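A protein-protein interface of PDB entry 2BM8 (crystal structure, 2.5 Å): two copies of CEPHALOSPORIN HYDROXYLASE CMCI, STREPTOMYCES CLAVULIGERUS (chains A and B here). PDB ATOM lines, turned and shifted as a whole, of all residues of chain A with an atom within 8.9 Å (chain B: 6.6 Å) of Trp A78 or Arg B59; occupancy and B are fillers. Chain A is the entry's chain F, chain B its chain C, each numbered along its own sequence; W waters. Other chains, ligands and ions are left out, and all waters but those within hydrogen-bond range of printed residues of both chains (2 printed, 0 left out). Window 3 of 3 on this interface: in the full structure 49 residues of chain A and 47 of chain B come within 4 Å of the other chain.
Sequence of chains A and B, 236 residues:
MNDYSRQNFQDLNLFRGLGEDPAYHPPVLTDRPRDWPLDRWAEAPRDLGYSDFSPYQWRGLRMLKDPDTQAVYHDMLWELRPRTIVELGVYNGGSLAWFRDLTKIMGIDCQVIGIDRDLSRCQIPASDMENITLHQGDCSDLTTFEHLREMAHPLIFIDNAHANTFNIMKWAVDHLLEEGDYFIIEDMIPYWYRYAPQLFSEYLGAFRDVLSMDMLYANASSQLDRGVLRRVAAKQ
NE2 of His A74 is in hydrogen-bond range of N of Arg B59, at 3.1 Å.
The side-chain amide nitrogen of Gln B57 sits close to the side-chain carboxylate of Asp A75, at 3.3 Å.
The guanidinium group of Arg B59 is in hydrogen-bond range of the backbone carbonyl oxygen of Ile A105 (3.0 Å).
Among the printed residues, merely in contact across the chains: Trp A78 with Arg B59, His A74 with Gln B57, His A74 with Trp B58, Trp A78 with Gly B60, Trp A78 with Gln B57, Ile A105 with Asp B101 and Leu A102 with Trp B58.
Water W2 bridges OD1 of Asp A75 (2.8 Å) and N of Gln B57 (3.2 Å).
Water W1 lies within hydrogen-bond range of NH1 of Arg B59 and O of Met A106.
Position printed for both chains: 101.
Of the 10 pairs that touch across the chains among the printed residues, none has its exchanged pair printed and touching as well.
Of the 23 printed residues of chain A, 5 touch a printed residue of chain B.
Hydrophobic or aromatic side chains of chain A within 4 Å of the printed part of chain B: His A74, Trp A78, Leu A102 and Ile A105.
Of the 12 printed residues of chain B, 5 touch a printed residue of chain A.
Among the printed residues, 10 pairs touch across the chains.
Among the printed residues, no Asp or Glu carboxylate lies within 4 Å of a Lys or Arg side-chain nitrogen of the other chain.
Trp A78 touches just these residues of chain B: Gln B57, Arg B59 and Gly B60.
Arg B59 touches just these residues of chain A: His A74 (3.1 Å), Trp A78 (3.3 Å) and Ile A105 (3.0 Å).
Of the printed residues of chain A, Gly B60 touches Trp A78.
Printed residues of chain B within 4 Å of Leu A102: Trp B58.
Of the printed residues of chain A, Asp B101 touches Ile A105.
Of the printed residues of chain A, Gln B57 touches His A74, Asp A75 and Trp A78.
Of the printed residues of chain B, His A74 touches Gln B57 (3.5 Å), Trp B58 (3.5 Å) and Arg B59 (3.1 Å).
Val A72 touches none of the printed residues of chain B.
The nearest residue of chain B that does not touch Trp A78 is Tyr B24 (5.4 Å).
The nearest printed residue of chain A that does not touch Asp B101 is Met A106 (7.1 Å).
The side-chain hydroxyl of Tyr B24 lies within hydrogen-bond range of the side-chain amide nitrogen of Gln B57, at 3.3 Å.
OE1 of Gln B57 lies within hydrogen-bond range of N of Gly B60.
The side-chain carboxylate (OD1) of Asp A75 is in hydrogen-bond range of a ring nitrogen (ND1) of His A74 (3.2 Å).
The guanidinium group of Arg B59 lies within salt-bridge range of the side-chain carboxylate of Asp B101.
The side-chain carboxylate of Asp B128 lies within salt-bridge range of the guanidinium group of Arg B59 (3.5 Å).
NE1 of Trp B58 sits at hydrogen-bond distance from OD2 of Asp B101.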
ATOM      1  N   ALA A  71      13.871 -13.383 -11.451  1.00  0.00           N
ATOM      2  CA  ALA A  71      13.336 -12.510 -12.461  1.00  0.00           C
ATOM      3  C   ALA A  71      14.029 -11.144 -12.426  1.00  0.00           C
ATOM      4  O   ALA A  71      14.273 -10.540 -13.463  1.00  0.00           O
ATOM      5  CB  ALA A  71      11.852 -12.375 -12.264  1.00  0.00           C
ATOM      6  N   VAL A  72      14.364 -10.673 -11.225  1.00  0.00           N
ATOM      7  CA  VAL A  72      15.132  -9.444 -11.068  1.00  0.00           C
ATOM      8  C   VAL A  72      16.542  -9.581 -11.614  1.00  0.00           C
ATOM      9  O   VAL A  72      17.000  -8.717 -12.330  1.00  0.00           O
ATOM     10  CB  VAL A  72      15.202  -8.993  -9.600  1.00  0.00           C
ATOM     11  CG1 VAL A  72      16.163  -7.816  -9.450  1.00  0.00           C
ATOM     12  CG2 VAL A  72      13.806  -8.619  -9.093  1.00  0.00           C
ATOM     13  N   TYR A  73      17.229 -10.671 -11.302  1.00  0.00           N
ATOM     14  CA  TYR A  73      18.590 -10.855 -11.809  1.00  0.00           C
ATOM     15  C   TYR A  73      18.605 -10.960 -13.336  1.00  0.00           C
ATOM     16  O   TYR A  73      19.491 -10.412 -13.978  1.00  0.00           O
ATOM     17  CB  TYR A  73      19.250 -12.071 -11.167  1.00  0.00           C
ATOM     18  CG  TYR A  73      19.855 -11.761  -9.827  1.00  0.00           C
ATOM     19  CD1 TYR A  73      19.403 -12.389  -8.679  1.00  0.00           C
ATOM     20  CD2 TYR A  73      20.869 -10.809  -9.706  1.00  0.00           C
ATOM     21  CE1 TYR A  73      19.941 -12.094  -7.441  1.00  0.00           C
ATOM     22  CE2 TYR A  73      21.425 -10.505  -8.480  1.00  0.00           C
ATOM     23  CZ  TYR A  73      20.961 -11.157  -7.346  1.00  0.00           C
ATOM     24  OH  TYR A  73      21.498 -10.853  -6.119  1.00  0.00           O
ATOM     25  N   HIS A  74      17.600 -11.615 -13.919  1.00  0.00           N
ATOM     26  CA  HIS A  74      17.496 -11.693 -15.373  1.00  0.00           C
ATOM     27  C   HIS A  74      17.391 -10.309 -16.002  1.00  0.00           C
ATOM     28  O   HIS A  74      18.073 -10.028 -16.983  1.00  0.00           O
ATOM     29  CB  HIS A  74      16.294 -12.529 -15.806  1.00  0.00           C
ATOM     30  CG  HIS A  74      16.026 -12.451 -17.269  1.00  0.00           C
ATOM     31  ND1 HIS A  74      15.430 -11.353 -17.859  1.00  0.00           N
ATOM     32  CD2 HIS A  74      16.310 -13.312 -18.271  1.00  0.00           C
ATOM     33  CE1 HIS A  74      15.365 -11.545 -19.163  1.00  0.00           C
ATOM     34  NE2 HIS A  74      15.894 -12.724 -19.439  1.00  0.00           N
ATOM     35  N   ASP A  75      16.542  -9.442 -15.459  1.00  0.00           N
ATOM     36  CA  ASP A  75      16.412  -8.087 -16.012  1.00  0.00           C
ATOM     37  C   ASP A  75      17.730  -7.328 -15.795  1.00  0.00           C
ATOM     38  O   ASP A  75      18.174  -6.601 -16.665  1.00  0.00           O
ATOM     39  CB  ASP A  75      15.223  -7.311 -15.408  1.00  0.00           C
ATOM     40  CG  ASP A  75      13.881  -8.038 -15.570  1.00  0.00           C
ATOM     41  OD1 ASP A  75      13.766  -8.994 -16.378  1.00  0.00           O
ATOM     42  OD2 ASP A  75      12.877  -7.745 -14.887  1.00  0.00           O
ATOM     43  N   MET A  76      18.363  -7.540 -14.647  1.00  0.00           N
ATOM     44  CA  MET A  76      19.611  -6.869 -14.314  1.00  0.00           C
ATOM     45  C   MET A  76      20.734  -7.334 -15.263  1.00  0.00           C
ATOM     46  O   MET A  76      21.451  -6.506 -15.828  1.00  0.00           O
ATOM     47  CB  MET A  76      19.990  -7.135 -12.853  1.00  0.00           C
ATOM     48  CG  MET A  76      21.201  -6.350 -12.376  1.00  0.00           C
ATOM     49  SD  MET A  76      21.600  -6.704 -10.656  1.00  0.00           S
ATOM     50  CE  MET A  76      20.070  -6.281  -9.867  1.00  0.00           C
ATOM     51  N   LEU A  77      20.848  -8.646 -15.464  1.00  0.00           N
ATOM     52  CA  LEU A  77      21.815  -9.186 -16.425  1.00  0.00           C
ATOM     53  C   LEU A  77      21.563  -8.687 -17.868  1.00  0.00           C
ATOM     54  O   LEU A  77      22.507  -8.404 -18.588  1.00  0.00           O
ATOM     55  CB  LEU A  77      21.848 -10.725 -16.382  1.00  0.00           C
ATOM     56  CG  LEU A  77      22.895 -11.415 -15.487  1.00  0.00           C
ATOM     57  CD1 LEU A  77      23.129 -10.735 -14.164  1.00  0.00           C
ATOM     58  CD2 LEU A  77      22.504 -12.847 -15.220  1.00  0.00           C
ATOM     59  N   TRP A  78      20.308  -8.554 -18.277  1.00  0.00           N
ATOM     60  CA  TRP A  78      19.981  -8.109 -19.633  1.00  0.00           C
ATOM     61  C   TRP A  78      20.303  -6.625 -19.873  1.00  0.00           C
ATOM     62  O   TRP A  78      20.731  -6.233 -20.958  1.00  0.00           O
ATOM     63  CB  TRP A  78      18.494  -8.381 -19.931  1.00  0.00           C
ATOM     64  CG  TRP A  78      18.144  -8.112 -21.328  1.00  0.00           C
ATOM     65  CD1 TRP A  78      17.469  -7.030 -21.810  1.00  0.00           C
ATOM     66  CD2 TRP A  78      18.482  -8.913 -22.453  1.00  0.00           C
ATOM     67  NE1 TRP A  78      17.362  -7.110 -23.177  1.00  0.00           N
ATOM     68  CE2 TRP A  78      17.977  -8.258 -23.603  1.00  0.00           C
ATOM     69  CE3 TRP A  78      19.174 -10.116 -22.616  1.00  0.00           C
ATOM     70  CZ2 TRP A  78      18.125  -8.778 -24.896  1.00  0.00           C
ATOM     71  CZ3 TRP A  78      19.325 -10.639 -23.905  1.00  0.00           C
ATOM     72  CH2 TRP A  78      18.798  -9.966 -25.027  1.00  0.00           C
ATOM     73  N   GLU A  79      20.127  -5.813 -18.840  1.00  0.00           N
ATOM     74  CA  GLU A  79      20.394  -4.382 -18.914  1.00  0.00           C
ATOM     75  C   GLU A  79      21.890  -4.072 -18.860  1.00  0.00           C
ATOM     76  O   GLU A  79      22.396  -3.257 -19.631  1.00  0.00           O
ATOM     77  CB  GLU A  79      19.669  -3.664 -17.760  1.00  0.00           C
ATOM     78  CG  GLU A  79      20.103  -2.230 -17.512  1.00  0.00           C
ATOM     79  CD  GLU A  79      19.188  -1.505 -16.543  1.00  0.00           C
ATOM     80  OE1 GLU A  79      18.845  -2.048 -15.470  1.00  0.00           O
ATOM     81  OE2 GLU A  79      18.813  -0.372 -16.864  1.00  0.00           O
ATOM     82  N   LEU A  80      22.578  -4.747 -17.945  1.00  0.00           N
ATOM     83  CA  LEU A  80      23.942  -4.410 -17.558  1.00  0.00           C
ATOM     84  C   LEU A  80      24.951  -5.209 -18.365  1.00  0.00           C
ATOM     85  O   LEU A  80      26.008  -4.707 -18.722  1.00  0.00           O
ATOM     86  CB  LEU A  80      24.125  -4.712 -16.074  1.00  0.00           C
ATOM     87  CG  LEU A  80      24.995  -3.839 -15.167  1.00  0.00           C
ATOM     88  CD1 LEU A  80      25.915  -4.764 -14.348  1.00  0.00           C
ATOM     89  CD2 LEU A  80      25.786  -2.721 -15.869  1.00  0.00           C
ATOM     90  N   ARG A  81      24.622  -6.474 -18.625  1.00  0.00           N
ATOM     91  CA  ARG A  81      25.527  -7.392 -19.325  1.00  0.00           C
ATOM     92  C   ARG A  81      26.894  -7.433 -18.642  1.00  0.00           C
ATOM     93  O   ARG A  81      27.892  -6.996 -19.210  1.00  0.00           O
ATOM     94  CB  ARG A  81      25.670  -6.985 -20.792  1.00  0.00           C
ATOM     95  CG  ARG A  81      24.358  -7.000 -21.557  1.00  0.00           C
ATOM     96  CD  ARG A  81      24.516  -6.587 -22.983  1.00  0.00           C
ATOM     97  NE  ARG A  81      25.271  -7.570 -23.756  1.00  0.00           N
ATOM     98  CZ  ARG A  81      24.769  -8.695 -24.259  1.00  0.00           C
ATOM     99  NH1 ARG A  81      23.496  -9.027 -24.066  1.00  0.00           N
ATOM    100  NH2 ARG A  81      25.551  -9.506 -24.955  1.00  0.00           N
ATOM    101  N   PRO A  82      26.930  -7.946 -17.416  1.00  0.00           N
ATOM    102  CA  PRO A  82      28.141  -7.920 -16.603  1.00  0.00           C
ATOM    103  C   PRO A  82      29.222  -8.868 -17.119  1.00  0.00           C
ATOM    104  O   PRO A  82      28.936 -10.013 -17.481  1.00  0.00           O
ATOM    105  CB  PRO A  82      27.636  -8.385 -15.245  1.00  0.00           C
ATOM    106  CG  PRO A  82      26.529  -9.317 -15.579  1.00  0.00           C
ATOM    107  CD  PRO A  82      25.826  -8.618 -16.703  1.00  0.00           C
ATOM    108  N   ILE A  85      30.328 -11.689 -12.337  1.00  0.00           N
ATOM    109  CA  ILE A  85      29.397 -11.815 -11.212  1.00  0.00           C
ATOM    110  C   ILE A  85      30.079 -12.577 -10.067  1.00  0.00           C
ATOM    111  O   ILE A  85      30.592 -13.668 -10.264  1.00  0.00           O
ATOM    112  CB  ILE A  85      28.137 -12.579 -11.645  1.00  0.00           C
ATOM    113  CG1 ILE A  85      27.315 -11.731 -12.613  1.00  0.00           C
ATOM    114  CG2 ILE A  85      27.273 -12.964 -10.427  1.00  0.00           C
ATOM    115  CD1 ILE A  85      26.331 -12.525 -13.407  1.00  0.00           C
ATOM    116  N   ASP A 101      24.841 -19.994 -16.796  1.00  0.00           N
ATOM    117  CA  ASP A 101      23.962 -20.444 -17.869  1.00  0.00           C
ATOM    118  C   ASP A 101      23.226 -19.281 -18.498  1.00  0.00           C
ATOM    119  O   ASP A 101      23.111 -19.214 -19.718  1.00  0.00           O
ATOM    120  CB  ASP A 101      22.937 -21.451 -17.359  1.00  0.00           C
ATOM    121  CG  ASP A 101      23.546 -22.802 -17.053  1.00  0.00           C
ATOM    122  OD1 ASP A 101      24.724 -23.061 -17.408  1.00  0.00           O
ATOM    123  OD2 ASP A 101      22.892 -23.675 -16.460  1.00  0.00           O
ATOM    124  N   LEU A 102      22.742 -18.364 -17.663  1.00  0.00           N
ATOM    125  CA  LEU A 102      21.949 -17.241 -18.127  1.00  0.00           C
ATOM    126  C   LEU A 102      22.801 -16.277 -18.945  1.00  0.00           C
ATOM    127  O   LEU A 102      22.330 -15.744 -19.949  1.00  0.00           O
ATOM    128  CB  LEU A 102      21.278 -16.518 -16.955  1.00  0.00           C
ATOM    129  CG  LEU A 102      19.801 -16.227 -17.187  1.00  0.00           C
ATOM    130  CD1 LEU A 102      18.989 -17.508 -16.999  1.00  0.00           C
ATOM    131  CD2 LEU A 102      19.324 -15.171 -16.257  1.00  0.00           C
ATOM    132  N   THR A 103      24.056 -16.069 -18.548  1.00  0.00           N
ATOM    133  CA  THR A 103      24.949 -15.184 -19.312  1.00  0.00           C
ATOM    134  C   THR A 103      25.342 -15.798 -20.657  1.00  0.00           C
ATOM    135  O   THR A 103      25.380 -15.114 -21.665  1.00  0.00           O
ATOM    136  CB  THR A 103      26.203 -14.778 -18.503  1.00  0.00           C
ATOM    137  OG1 THR A 103      26.668 -15.867 -17.695  1.00  0.00           O
ATOM    138  CG2 THR A 103      25.855 -13.702 -17.499  1.00  0.00           C
ATOM    139  N   LYS A 104      25.612 -17.092 -20.685  1.00  0.00           N
ATOM    140  CA  LYS A 104      25.864 -17.788 -21.949  1.00  0.00           C
ATOM    141  C   LYS A 104      24.674 -17.631 -22.905  1.00  0.00           C
ATOM    142  O   LYS A 104      24.852 -17.310 -24.070  1.00  0.00           O
ATOM    143  CB  LYS A 104      26.158 -19.271 -21.678  1.00  0.00           C
ATOM    144  CG  LYS A 104      26.642 -20.071 -22.858  1.00  0.00           C
ATOM    145  CD  LYS A 104      26.774 -21.583 -22.491  1.00  0.00           C
ATOM    146  CE  LYS A 104      28.193 -22.156 -22.774  1.00  0.00           C
ATOM    147  NZ  LYS A 104      29.143 -21.938 -21.615  1.00  0.00           N
ATOM    148  N   ILE A 105      23.461 -17.831 -22.404  1.00  0.00           N
ATOM    149  CA  ILE A 105      22.277 -17.748 -23.254  1.00  0.00           C
ATOM    150  C   ILE A 105      22.080 -16.330 -23.800  1.00  0.00           C
ATOM    151  O   ILE A 105      21.588 -16.166 -24.896  1.00  0.00           O
ATOM    152  CB  ILE A 105      21.006 -18.210 -22.521  1.00  0.00           C
ATOM    153  CG1 ILE A 105      21.117 -19.677 -22.114  1.00  0.00           C
ATOM    154  CG2 ILE A 105      19.820 -18.110 -23.446  1.00  0.00           C
ATOM    155  CD1 ILE A 105      19.947 -20.171 -21.218  1.00  0.00           C
ATOM    156  N   MET A 106      22.488 -15.317 -23.049  1.00  0.00           N
ATOM    157  CA  MET A 106      22.338 -13.936 -23.488  1.00  0.00           C
ATOM    158  C   MET A 106      23.490 -13.478 -24.385  1.00  0.00           C
ATOM    159  O   MET A 106      23.482 -12.344 -24.889  1.00  0.00           O
ATOM    160  CB  MET A 106      22.220 -13.005 -22.277  1.00  0.00           C
ATOM    161  CG  MET A 106      20.970 -13.220 -21.434  1.00  0.00           C
ATOM    162  SD  MET A 106      20.960 -12.184 -19.935  1.00  0.00           S
ATOM    163  CE  MET A 106      19.384 -12.622 -19.249  1.00  0.00           C
ATOM    164  N   GLY A 107      24.482 -14.342 -24.581  1.00  0.00           N
ATOM    165  CA  GLY A 107      25.642 -14.003 -25.394  1.00  0.00           C
ATOM    166  C   GLY A 107      26.622 -13.083 -24.679  1.00  0.00           C
ATOM    167  O   GLY A 107      27.421 -12.418 -25.341  1.00  0.00           O
ATOM    168  N   ILE A 108      26.568 -13.057 -23.339  1.00  0.00           N
ATOM    169  CA  ILE A 108      27.462 -12.237 -22.502  1.00  0.00           C
ATOM    170  C   ILE A 108      28.716 -13.015 -22.086  1.00  0.00           C
ATOM    171  O   ILE A 108      28.640 -14.175 -21.681  1.00  0.00           O
ATOM    172  CB  ILE A 108      26.733 -11.712 -21.227  1.00  0.00           C
ATOM    173  CG1 ILE A 108      25.363 -11.119 -21.581  1.00  0.00           C
ATOM    174  CG2 ILE A 108      27.570 -10.632 -20.530  1.00  0.00           C
ATOM    175  CD1 ILE A 108      24.492 -10.766 -20.387  1.00  0.00           C
ATOM    176  N   ILE A 156      28.841  -7.297 -10.850  1.00  0.00           N
ATOM    177  CA  ILE A 156      27.795  -7.412  -9.819  1.00  0.00           C
ATOM    178  C   ILE A 156      28.422  -8.199  -8.667  1.00  0.00           C
ATOM    179  O   ILE A 156      28.885  -9.315  -8.887  1.00  0.00           O
ATOM    180  CB  ILE A 156      26.555  -8.186 -10.358  1.00  0.00           C
ATOM    181  CG1 ILE A 156      25.850  -7.423 -11.472  1.00  0.00           C
ATOM    182  CG2 ILE A 156      25.557  -8.482  -9.247  1.00  0.00           C
ATOM    183  CD1 ILE A 156      24.905  -8.287 -12.265  1.00  0.00           C
ATOM    184  N   TYR A 217      14.941  -2.206  -9.024  1.00  0.00           N
ATOM    185  CA  TYR A 217      15.072  -3.598  -8.561  1.00  0.00           C
ATOM    186  C   TYR A 217      14.881  -3.812  -7.068  1.00  0.00           C
ATOM    187  O   TYR A 217      14.584  -4.929  -6.636  1.00  0.00           O
ATOM    188  CB  TYR A 217      16.438  -4.132  -8.957  1.00  0.00           C
ATOM    189  CG  TYR A 217      16.709  -4.061 -10.440  1.00  0.00           C
ATOM    190  CD1 TYR A 217      17.877  -3.478 -10.927  1.00  0.00           C
ATOM    191  CD2 TYR A 217      15.809  -4.599 -11.357  1.00  0.00           C
ATOM    192  CE1 TYR A 217      18.143  -3.424 -12.302  1.00  0.00           C
ATOM    193  CE2 TYR A 217      16.055  -4.556 -12.735  1.00  0.00           C
ATOM    194  CZ  TYR A 217      17.219  -3.956 -13.202  1.00  0.00           C
ATOM    195  OH  TYR A 217      17.460  -3.912 -14.553  1.00  0.00           O
ATOM    196  N   TYR B  24       8.836  -5.694 -25.989  1.00  0.00           N
ATOM    197  CA  TYR B  24       9.179  -5.422 -24.594  1.00  0.00           C
ATOM    198  C   TYR B  24       9.714  -4.011 -24.431  1.00  0.00           C
ATOM    199  O   TYR B  24      10.514  -3.545 -25.246  1.00  0.00           O
ATOM    200  CB  TYR B  24      10.249  -6.400 -24.066  1.00  0.00           C
ATOM    201  CG  TYR B  24      10.724  -6.082 -22.637  1.00  0.00           C
ATOM    202  CD1 TYR B  24       9.896  -6.300 -21.533  1.00  0.00           C
ATOM    203  CD2 TYR B  24      11.994  -5.554 -22.401  1.00  0.00           C
ATOM    204  CE1 TYR B  24      10.317  -6.001 -20.245  1.00  0.00           C
ATOM    205  CE2 TYR B  24      12.438  -5.261 -21.098  1.00  0.00           C
ATOM    206  CZ  TYR B  24      11.594  -5.482 -20.034  1.00  0.00           C
ATOM    207  OH  TYR B  24      12.022  -5.185 -18.751  1.00  0.00           O
ATOM    208  N   GLN B  57       9.985 -10.438 -18.775  1.00  0.00           N
ATOM    209  CA  GLN B  57      10.654 -10.609 -20.048  1.00  0.00           C
ATOM    210  C   GLN B  57      11.568 -11.832 -20.035  1.00  0.00           C
ATOM    211  O   GLN B  57      11.892 -12.386 -18.975  1.00  0.00           O
ATOM    212  CB  GLN B  57      11.494  -9.368 -20.374  1.00  0.00           C
ATOM    213  CG  GLN B  57      12.590  -9.080 -19.348  1.00  0.00           C
ATOM    214  CD  GLN B  57      13.824  -8.423 -19.938  1.00  0.00           C
ATOM    215  OE1 GLN B  57      14.258  -8.768 -21.023  1.00  0.00           O
ATOM    216  NE2 GLN B  57      14.389  -7.484 -19.213  1.00  0.00           N
ATOM    217  N   TRP B  58      11.977 -12.218 -21.239  1.00  0.00           N
ATOM    218  CA  TRP B  58      13.031 -13.172 -21.456  1.00  0.00           C
ATOM    219  C   TRP B  58      13.853 -12.675 -22.649  1.00  0.00           C
ATOM    220  O   TRP B  58      13.356 -12.608 -23.765  1.00  0.00           O
ATOM    221  CB  TRP B  58      12.424 -14.564 -21.714  1.00  0.00           C
ATOM    222  CG  TRP B  58      13.431 -15.568 -22.036  1.00  0.00           C
ATOM    223  CD1 TRP B  58      13.725 -16.059 -23.266  1.00  0.00           C
ATOM    224  CD2 TRP B  58      14.346 -16.178 -21.127  1.00  0.00           C
ATOM    225  NE1 TRP B  58      14.751 -16.971 -23.179  1.00  0.00           N
ATOM    226  CE2 TRP B  58      15.149 -17.064 -21.870  1.00  0.00           C
ATOM    227  CE3 TRP B  58      14.549 -16.090 -19.745  1.00  0.00           C
ATOM    228  CZ2 TRP B  58      16.151 -17.828 -21.290  1.00  0.00           C
ATOM    229  CZ3 TRP B  58      15.530 -16.861 -19.169  1.00  0.00           C
ATOM    230  CH2 TRP B  58      16.330 -17.711 -19.942  1.00  0.00           C
ATOM    231  N   ARG B  59      15.099 -12.290 -22.394  1.00  0.00           N
ATOM    232  CA  ARG B  59      16.018 -11.805 -23.426  1.00  0.00           C
ATOM    233  C   ARG B  59      15.442 -10.746 -24.346  1.00  0.00           C
ATOM    234  O   ARG B  59      15.585 -10.835 -25.553  1.00  0.00           O
ATOM    235  CB  ARG B  59      16.484 -12.981 -24.267  1.00  0.00           C
ATOM    236  CG  ARG B  59      17.000 -14.125 -23.443  1.00  0.00           C
ATOM    237  CD  ARG B  59      18.166 -14.820 -24.081  1.00  0.00           C
ATOM    238  NE  ARG B  59      17.722 -15.770 -25.087  1.00  0.00           N
ATOM    239  CZ  ARG B  59      18.273 -15.960 -26.284  1.00  0.00           C
ATOM    240  NH1 ARG B  59      19.308 -15.241 -26.697  1.00  0.00           N
ATOM    241  NH2 ARG B  59      17.764 -16.889 -27.088  1.00  0.00           N
ATOM    242  N   GLY B  60      14.777  -9.752 -23.773  1.00  0.00           N
ATOM    243  CA  GLY B  60      14.227  -8.656 -24.545  1.00  0.00           C
ATOM    244  C   GLY B  60      12.877  -8.935 -25.187  1.00  0.00           C
ATOM    245  O   GLY B  60      12.361  -8.083 -25.907  1.00  0.00           O
ATOM    246  N   LEU B  61      12.297 -10.103 -24.914  1.00  0.00           N
ATOM    247  CA  LEU B  61      10.971 -10.455 -25.400  1.00  0.00           C
ATOM    248  C   LEU B  61      10.022 -10.471 -24.224  1.00  0.00           C
ATOM    249  O   LEU B  61      10.380 -10.968 -23.154  1.00  0.00           O
ATOM    250  CB  LEU B  61      10.986 -11.853 -26.007  1.00  0.00           C
ATOM    251  CG  LEU B  61      12.037 -12.184 -27.062  1.00  0.00           C
ATOM    252  CD1 LEU B  61      12.043 -13.682 -27.377  1.00  0.00           C
ATOM    253  CD2 LEU B  61      11.807 -11.371 -28.319  1.00  0.00           C
ATOM    254  N   MET B  63       7.351 -11.779 -21.654  1.00  0.00           N
ATOM    255  CA  MET B  63       7.036 -13.100 -21.101  1.00  0.00           C
ATOM    256  C   MET B  63       5.733 -12.996 -20.326  1.00  0.00           C
ATOM    257  O   MET B  63       5.694 -12.349 -19.288  1.00  0.00           O
ATOM    258  CB  MET B  63       8.125 -13.547 -20.123  1.00  0.00           C
ATOM    259  CG  MET B  63       9.172 -14.483 -20.687  1.00  0.00           C
ATOM    260  SD  MET B  63       8.536 -16.111 -21.132  1.00  0.00           S
ATOM    261  CE  MET B  63       7.703 -16.520 -19.767  1.00  0.00           C
ATOM    262  N   ALA B  97      10.370 -18.993 -27.277  1.00  0.00           N
ATOM    263  CA  ALA B  97      11.816 -18.756 -27.220  1.00  0.00           C
ATOM    264  C   ALA B  97      12.396 -19.224 -25.893  1.00  0.00           C
ATOM    265  O   ALA B  97      13.481 -19.785 -25.844  1.00  0.00           O
ATOM    266  CB  ALA B  97      12.123 -17.270 -27.435  1.00  0.00           C
ATOM    267  N   ARG B 100      12.288 -23.250 -25.857  1.00  0.00           N
ATOM    268  CA  ARG B 100      13.408 -23.679 -26.687  1.00  0.00           C
ATOM    269  C   ARG B 100      14.755 -23.450 -25.972  1.00  0.00           C
ATOM    270  O   ARG B 100      15.575 -24.357 -25.937  1.00  0.00           O
ATOM    271  CB  ARG B 100      13.372 -22.934 -28.029  1.00  0.00           C
ATOM    272  CG  ARG B 100      14.362 -23.440 -29.091  1.00  0.00           C
ATOM    273  CD  ARG B 100      15.794 -22.845 -29.054  1.00  0.00           C
ATOM    274  NE  ARG B 100      15.822 -21.440 -28.686  1.00  0.00           N
ATOM    275  CZ  ARG B 100      15.617 -20.414 -29.512  1.00  0.00           C
ATOM    276  NH1 ARG B 100      15.364 -20.597 -30.804  1.00  0.00           N
ATOM    277  NH2 ARG B 100      15.646 -19.175 -29.023  1.00  0.00           N
ATOM    278  N   ASP B 101      14.977 -22.261 -25.398  1.00  0.00           N
ATOM    279  CA  ASP B 101      16.245 -21.953 -24.715  1.00  0.00           C
ATOM    280  C   ASP B 101      16.467 -22.863 -23.526  1.00  0.00           C
ATOM    281  O   ASP B 101      17.576 -23.300 -23.276  1.00  0.00           O
ATOM    282  CB  ASP B 101      16.291 -20.509 -24.195  1.00  0.00           C
ATOM    283  CG  ASP B 101      16.471 -19.496 -25.286  1.00  0.00           C
ATOM    284  OD1 ASP B 101      16.771 -19.882 -26.433  1.00  0.00           O
ATOM    285  OD2 ASP B 101      16.317 -18.274 -25.094  1.00  0.00           O
ATOM    286  N   PRO B 125      13.616 -12.469 -32.928  1.00  0.00           N
ATOM    287  CA  PRO B 125      14.547 -12.160 -34.027  1.00  0.00           C
ATOM    288  C   PRO B 125      14.781 -13.373 -34.923  1.00  0.00           C
ATOM    289  O   PRO B 125      14.789 -14.515 -34.451  1.00  0.00           O
ATOM    290  CB  PRO B 125      15.826 -11.740 -33.313  1.00  0.00           C
ATOM    291  CG  PRO B 125      15.363 -11.244 -31.984  1.00  0.00           C
ATOM    292  CD  PRO B 125      14.180 -12.102 -31.614  1.00  0.00           C
ATOM    293  N   ASP B 128      17.538 -15.952 -34.155  1.00  0.00           N
ATOM    294  CA  ASP B 128      17.345 -17.123 -33.282  1.00  0.00           C
ATOM    295  C   ASP B 128      15.960 -17.754 -33.263  1.00  0.00           C
ATOM    296  O   ASP B 128      15.326 -17.861 -32.229  1.00  0.00           O
ATOM    297  CB  ASP B 128      17.895 -16.905 -31.866  1.00  0.00           C
ATOM    298  CG  ASP B 128      17.306 -15.708 -31.171  1.00  0.00           C
ATOM    299  OD1 ASP B 128      16.550 -15.941 -30.187  1.00  0.00           O
ATOM    300  OD2 ASP B 128      17.595 -14.518 -31.492  1.00  0.00           O
HETATM  301  O   HOH W   1      20.648 -12.700 -26.231  1.00  0.00           O
HETATM  302  O   HOH W   2      11.624 -10.727 -15.990  1.00  0.00           O
